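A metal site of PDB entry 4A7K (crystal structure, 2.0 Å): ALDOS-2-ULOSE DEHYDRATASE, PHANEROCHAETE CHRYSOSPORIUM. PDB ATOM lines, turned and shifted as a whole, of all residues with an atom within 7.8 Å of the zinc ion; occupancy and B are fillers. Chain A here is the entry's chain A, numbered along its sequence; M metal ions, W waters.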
ATOM      1  N   GLY A 628     -31.273 -15.383   6.967  1.00  0.00           N
ATOM      2  CA  GLY A 628     -32.560 -15.787   7.501  1.00  0.00           C
ATOM      3  C   GLY A 628     -32.741 -15.510   9.002  1.00  0.00           C
ATOM      4  O   GLY A 628     -31.881 -15.882   9.886  1.00  0.00           O
ATOM      5  N   PHE A 629     -33.892 -14.870   9.315  1.00  0.00           N
ATOM      6  CA  PHE A 629     -34.248 -14.586  10.728  1.00  0.00           C
ATOM      7  C   PHE A 629     -34.531 -15.847  11.545  1.00  0.00           C
ATOM      8  O   PHE A 629     -35.243 -16.743  11.072  1.00  0.00           O
ATOM      9  CB  PHE A 629     -35.421 -13.603  10.755  1.00  0.00           C
ATOM     10  CG  PHE A 629     -35.015 -12.206  10.465  1.00  0.00           C
ATOM     11  CD1 PHE A 629     -34.562 -11.400  11.484  1.00  0.00           C
ATOM     12  CD2 PHE A 629     -34.998 -11.720   9.140  1.00  0.00           C
ATOM     13  CE1 PHE A 629     -34.148 -10.103  11.225  1.00  0.00           C
ATOM     14  CE2 PHE A 629     -34.577 -10.445   8.875  1.00  0.00           C
ATOM     15  CZ  PHE A 629     -34.138  -9.620   9.924  1.00  0.00           C
ATOM     16  N   HIS A 630     -33.965 -15.931  12.754  1.00  0.00           N
ATOM     17  CA  HIS A 630     -34.128 -17.145  13.596  1.00  0.00           C
ATOM     18  C   HIS A 630     -33.931 -16.659  15.000  1.00  0.00           C
ATOM     19  O   HIS A 630     -33.669 -15.450  15.235  1.00  0.00           O
ATOM     20  CB  HIS A 630     -33.086 -18.211  13.180  1.00  0.00           C
ATOM     21  CG  HIS A 630     -31.685 -17.714  13.347  1.00  0.00           C
ATOM     22  ND1 HIS A 630     -31.076 -16.903  12.428  1.00  0.00           N
ATOM     23  CD2 HIS A 630     -30.832 -17.775  14.431  1.00  0.00           C
ATOM     24  CE1 HIS A 630     -29.871 -16.520  12.903  1.00  0.00           C
ATOM     25  NE2 HIS A 630     -29.720 -17.073  14.121  1.00  0.00           N
ATOM     26  N   ASN A 631     -34.098 -17.567  15.966  1.00  0.00           N
ATOM     27  CA  ASN A 631     -34.109 -17.185  17.391  1.00  0.00           C
ATOM     28  C   ASN A 631     -33.549 -18.235  18.325  1.00  0.00           C
ATOM     29  O   ASN A 631     -33.639 -18.063  19.542  1.00  0.00           O
ATOM     30  CB  ASN A 631     -35.528 -16.778  17.853  1.00  0.00           C
ATOM     31  CG  ASN A 631     -36.495 -17.990  17.947  1.00  0.00           C
ATOM     32  OD1 ASN A 631     -36.165 -19.115  17.507  1.00  0.00           O
ATOM     33  ND2 ASN A 631     -37.700 -17.746  18.422  1.00  0.00           N
ATOM     34  N   HIS A 632     -32.956 -19.321  17.799  1.00  0.00           N
ATOM     35  CA  HIS A 632     -32.250 -20.336  18.652  1.00  0.00           C
ATOM     36  C   HIS A 632     -33.116 -21.008  19.679  1.00  0.00           C
ATOM     37  O   HIS A 632     -32.640 -21.307  20.816  1.00  0.00           O
ATOM     38  CB  HIS A 632     -30.942 -19.760  19.324  1.00  0.00           C
ATOM     39  CG  HIS A 632     -30.010 -19.185  18.306  1.00  0.00           C
ATOM     40  ND1 HIS A 632     -29.462 -19.960  17.310  1.00  0.00           N
ATOM     41  CD2 HIS A 632     -29.594 -17.863  18.073  1.00  0.00           C
ATOM     42  CE1 HIS A 632     -28.705 -19.120  16.509  1.00  0.00           C
ATOM     43  NE2 HIS A 632     -28.797 -17.866  16.991  1.00  0.00           N
ATOM     44  N   PHE A 637     -27.530 -21.490  23.161  1.00  0.00           N
ATOM     45  CA  PHE A 637     -26.172 -20.980  23.328  1.00  0.00           C
ATOM     46  C   PHE A 637     -26.121 -19.427  23.223  1.00  0.00           C
ATOM     47  O   PHE A 637     -27.100 -18.839  22.832  1.00  0.00           O
ATOM     48  CB  PHE A 637     -25.221 -21.655  22.321  1.00  0.00           C
ATOM     49  CG  PHE A 637     -25.705 -21.575  20.855  1.00  0.00           C
ATOM     50  CD1 PHE A 637     -25.693 -20.364  20.154  1.00  0.00           C
ATOM     51  CD2 PHE A 637     -26.125 -22.720  20.200  1.00  0.00           C
ATOM     52  CE1 PHE A 637     -26.127 -20.323  18.839  1.00  0.00           C
ATOM     53  CE2 PHE A 637     -26.542 -22.683  18.871  1.00  0.00           C
ATOM     54  CZ  PHE A 637     -26.577 -21.490  18.211  1.00  0.00           C
ATOM     55  N   GLU A 639     -24.334 -16.516  21.386  1.00  0.00           N
ATOM     56  CA  GLU A 639     -23.475 -16.402  20.194  1.00  0.00           C
ATOM     57  C   GLU A 639     -22.922 -15.011  19.956  1.00  0.00           C
ATOM     58  O   GLU A 639     -23.578 -13.968  20.156  1.00  0.00           O
ATOM     59  CB  GLU A 639     -24.181 -16.911  18.906  1.00  0.00           C
ATOM     60  CG  GLU A 639     -25.444 -16.195  18.548  1.00  0.00           C
ATOM     61  CD  GLU A 639     -25.955 -16.481  17.137  1.00  0.00           C
ATOM     62  OE1 GLU A 639     -25.559 -17.477  16.483  1.00  0.00           O
ATOM     63  OE2 GLU A 639     -26.817 -15.666  16.676  1.00  0.00           O
ATOM     64  N   HIS A 641     -20.635 -12.997  16.780  1.00  0.00           N
ATOM     65  CA  HIS A 641     -20.058 -13.130  15.455  1.00  0.00           C
ATOM     66  C   HIS A 641     -18.935 -12.148  15.290  1.00  0.00           C
ATOM     67  O   HIS A 641     -19.014 -11.040  15.772  1.00  0.00           O
ATOM     68  CB  HIS A 641     -21.109 -12.888  14.366  1.00  0.00           C
ATOM     69  CG  HIS A 641     -22.280 -13.840  14.431  1.00  0.00           C
ATOM     70  ND1 HIS A 641     -23.466 -13.480  14.943  1.00  0.00           N
ATOM     71  CD2 HIS A 641     -22.391 -15.183  14.075  1.00  0.00           C
ATOM     72  CE1 HIS A 641     -24.315 -14.528  14.889  1.00  0.00           C
ATOM     73  NE2 HIS A 641     -23.682 -15.556  14.332  1.00  0.00           N
ATOM     74  N   MET A 653     -25.700  -7.390  11.391  1.00  0.00           N
ATOM     75  CA  MET A 653     -26.787  -8.037  12.159  1.00  0.00           C
ATOM     76  C   MET A 653     -27.975  -7.126  12.299  1.00  0.00           C
ATOM     77  O   MET A 653     -27.846  -5.926  12.601  1.00  0.00           O
ATOM     78  CB  MET A 653     -26.298  -8.466  13.546  1.00  0.00           C
ATOM     79  CG  MET A 653     -25.096  -9.445  13.458  1.00  0.00           C
ATOM     80  SD  MET A 653     -25.537 -11.092  12.824  1.00  0.00           S
ATOM     81  CE  MET A 653     -26.740 -11.734  13.986  1.00  0.00           C
ATOM     82  N   HIS A 684     -19.379  -8.174  17.093  1.00  0.00           N
ATOM     83  CA  HIS A 684     -20.538  -7.385  17.629  1.00  0.00           C
ATOM     84  C   HIS A 684     -20.843  -7.919  19.023  1.00  0.00           C
ATOM     85  O   HIS A 684     -20.428  -9.023  19.332  1.00  0.00           O
ATOM     86  CB  HIS A 684     -21.762  -7.449  16.700  1.00  0.00           C
ATOM     87  CG  HIS A 684     -22.434  -8.815  16.739  1.00  0.00           C
ATOM     88  ND1 HIS A 684     -23.162  -9.238  17.799  1.00  0.00           N
ATOM     89  CD2 HIS A 684     -22.430  -9.865  15.826  1.00  0.00           C
ATOM     90  CE1 HIS A 684     -23.606 -10.493  17.581  1.00  0.00           C
ATOM     91  NE2 HIS A 684     -23.176 -10.875  16.353  1.00  0.00           N
ATOM     92  N   LEU A 687     -26.874 -10.078  21.345  1.00  0.00           N
ATOM     93  CA  LEU A 687     -28.187  -9.629  20.916  1.00  0.00           C
ATOM     94  C   LEU A 687     -29.261 -10.423  21.653  1.00  0.00           C
ATOM     95  O   LEU A 687     -30.448 -10.149  21.507  1.00  0.00           O
ATOM     96  CB  LEU A 687     -28.347  -9.833  19.431  1.00  0.00           C
ATOM     97  CG  LEU A 687     -27.248  -9.274  18.561  1.00  0.00           C
ATOM     98  CD1 LEU A 687     -27.508  -9.625  17.087  1.00  0.00           C
ATOM     99  CD2 LEU A 687     -27.187  -7.765  18.737  1.00  0.00           C
ATOM    100  N   TYR A 706     -33.736 -15.135  22.380  1.00  0.00           N
ATOM    101  CA  TYR A 706     -33.279 -14.109  21.447  1.00  0.00           C
ATOM    102  C   TYR A 706     -34.471 -13.501  20.794  1.00  0.00           C
ATOM    103  O   TYR A 706     -35.487 -14.224  20.539  1.00  0.00           O
ATOM    104  CB  TYR A 706     -32.505 -14.734  20.307  1.00  0.00           C
ATOM    105  CG  TYR A 706     -31.125 -15.223  20.656  1.00  0.00           C
ATOM    106  CD1 TYR A 706     -30.952 -16.422  21.409  1.00  0.00           C
ATOM    107  CD2 TYR A 706     -30.008 -14.554  20.198  1.00  0.00           C
ATOM    108  CE1 TYR A 706     -29.674 -16.929  21.667  1.00  0.00           C
ATOM    109  CE2 TYR A 706     -28.716 -15.027  20.464  1.00  0.00           C
ATOM    110  CZ  TYR A 706     -28.556 -16.174  21.253  1.00  0.00           C
ATOM    111  OH  TYR A 706     -27.270 -16.669  21.450  1.00  0.00           O
ATOM    112  N   PRO A 707     -34.414 -12.181  20.510  1.00  0.00           N
ATOM    113  CA  PRO A 707     -35.361 -11.647  19.547  1.00  0.00           C
ATOM    114  C   PRO A 707     -35.010 -12.253  18.168  1.00  0.00           C
ATOM    115  O   PRO A 707     -33.922 -12.837  18.011  1.00  0.00           O
ATOM    116  CB  PRO A 707     -35.015 -10.166  19.558  1.00  0.00           C
ATOM    117  CG  PRO A 707     -33.498 -10.170  19.729  1.00  0.00           C
ATOM    118  CD  PRO A 707     -33.273 -11.252  20.749  1.00  0.00           C
ATOM    119  N   TRP A 708     -35.942 -12.193  17.205  1.00  0.00           N
ATOM    120  CA  TRP A 708     -35.643 -12.609  15.846  1.00  0.00           C
ATOM    121  C   TRP A 708     -34.463 -11.786  15.373  1.00  0.00           C
ATOM    122  O   TRP A 708     -34.432 -10.556  15.575  1.00  0.00           O
ATOM    123  CB  TRP A 708     -36.859 -12.308  14.942  1.00  0.00           C
ATOM    124  CG  TRP A 708     -38.103 -13.127  15.225  1.00  0.00           C
ATOM    125  CD1 TRP A 708     -39.348 -12.684  15.672  1.00  0.00           C
ATOM    126  CD2 TRP A 708     -38.261 -14.571  14.985  1.00  0.00           C
ATOM    127  NE1 TRP A 708     -40.224 -13.727  15.761  1.00  0.00           N
ATOM    128  CE2 TRP A 708     -39.632 -14.895  15.341  1.00  0.00           C
ATOM    129  CE3 TRP A 708     -37.414 -15.582  14.510  1.00  0.00           C
ATOM    130  CZ2 TRP A 708     -40.121 -16.194  15.240  1.00  0.00           C
ATOM    131  CZ3 TRP A 708     -37.924 -16.890  14.436  1.00  0.00           C
ATOM    132  CH2 TRP A 708     -39.241 -17.174  14.790  1.00  0.00           C
ATOM    133  N   HIS A 709     -33.508 -12.429  14.692  1.00  0.00           N
ATOM    134  CA  HIS A 709     -32.260 -11.739  14.266  1.00  0.00           C
ATOM    135  C   HIS A 709     -31.628 -12.516  13.102  1.00  0.00           C
ATOM    136  O   HIS A 709     -31.964 -13.674  12.854  1.00  0.00           O
ATOM    137  CB  HIS A 709     -31.254 -11.560  15.436  1.00  0.00           C
ATOM    138  CG  HIS A 709     -30.751 -12.873  15.966  1.00  0.00           C
ATOM    139  ND1 HIS A 709     -31.531 -13.681  16.719  1.00  0.00           N
ATOM    140  CD2 HIS A 709     -29.613 -13.607  15.656  1.00  0.00           C
ATOM    141  CE1 HIS A 709     -30.878 -14.864  16.959  1.00  0.00           C
ATOM    142  NE2 HIS A 709     -29.716 -14.825  16.308  1.00  0.00           N
ATOM    143  N   ALA A 710     -30.731 -11.866  12.339  1.00  0.00           N
ATOM    144  CA  ALA A 710     -30.135 -12.498  11.183  1.00  0.00           C
ATOM    145  C   ALA A 710     -28.933 -11.679  10.800  1.00  0.00           C
ATOM    146  O   ALA A 710     -28.896 -10.476  11.093  1.00  0.00           O
ATOM    147  CB  ALA A 710     -31.142 -12.503  10.028  1.00  0.00           C
ATOM    148  N   TRP A 711     -27.926 -12.315  10.172  1.00  0.00           N
ATOM    149  CA  TRP A 711     -26.917 -11.588   9.389  1.00  0.00           C
ATOM    150  C   TRP A 711     -27.580 -11.338   8.044  1.00  0.00           C
ATOM    151  O   TRP A 711     -28.160 -12.294   7.462  1.00  0.00           O
ATOM    152  CB  TRP A 711     -25.586 -12.409   9.223  1.00  0.00           C
ATOM    153  CG  TRP A 711     -24.552 -11.641   8.403  1.00  0.00           C
ATOM    154  CD1 TRP A 711     -24.558 -11.373   7.023  1.00  0.00           C
ATOM    155  CD2 TRP A 711     -23.380 -10.906   8.920  1.00  0.00           C
ATOM    156  NE1 TRP A 711     -23.491 -10.555   6.658  1.00  0.00           N
ATOM    157  CE2 TRP A 711     -22.748 -10.256   7.771  1.00  0.00           C
ATOM    158  CE3 TRP A 711     -22.816 -10.755  10.193  1.00  0.00           C
ATOM    159  CZ2 TRP A 711     -21.579  -9.487   7.913  1.00  0.00           C
ATOM    160  CZ3 TRP A 711     -21.639  -9.958  10.308  1.00  0.00           C
ATOM    161  CH2 TRP A 711     -21.062  -9.354   9.197  1.00  0.00           C
ATOM    162  N   ALA A 728     -18.899 -17.627  13.520  1.00  0.00           N
ATOM    163  CA  ALA A 728     -19.776 -17.772  14.689  1.00  0.00           C
ATOM    164  C   ALA A 728     -19.045 -18.426  15.890  1.00  0.00           C
ATOM    165  O   ALA A 728     -18.400 -19.477  15.736  1.00  0.00           O
ATOM    166  CB  ALA A 728     -21.032 -18.555  14.361  1.00  0.00           C
HETATM  167 ZN    ZN M   1     -28.366 -16.336  15.587  1.00  0.00          ZN
HETATM  168  O   HOH W   1     -27.143 -15.206  13.877  1.00  0.00           O
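OE2 of Glu 639 binds the zinc ion, 2.0 Å away.
A ring nitrogen (NE2) of His 632 is bound to the zinc ion (2.1 Å).
The zinc ion is bound by NE2 of His 630, 2.1 Å away.
The zinc ion is bound by a ring nitrogen (NE2) of His 709 (2.2 Å).
The zinc ion is bound by water W1 (2.4 Å).
The zinc ion has five donor atoms within binding distance.
The backbone NH (N) of Glu 639 sits at hydrogen-bond distance from the side-chain hydroxyl (OH) of Tyr 706, at 2.9 Å.
The backbone carbonyl oxygen (O) of Pro 707 sits at hydrogen-bond distance from a ring nitrogen (ND1) of His 709.
The side-chain carboxylate (OE1) of Glu 639 sits at hydrogen-bond distance from a ring nitrogen (NE2) of His 641 (3.4 Å).
The backbone carbonyl oxygen (O) of Gly 628 sits at hydrogen-bond distance from a ring nitrogen (ND1) of His 630, at 2.9 Å.
The nearest printed residue that does not touch the zinc ion is His 641 (4.5 Å).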
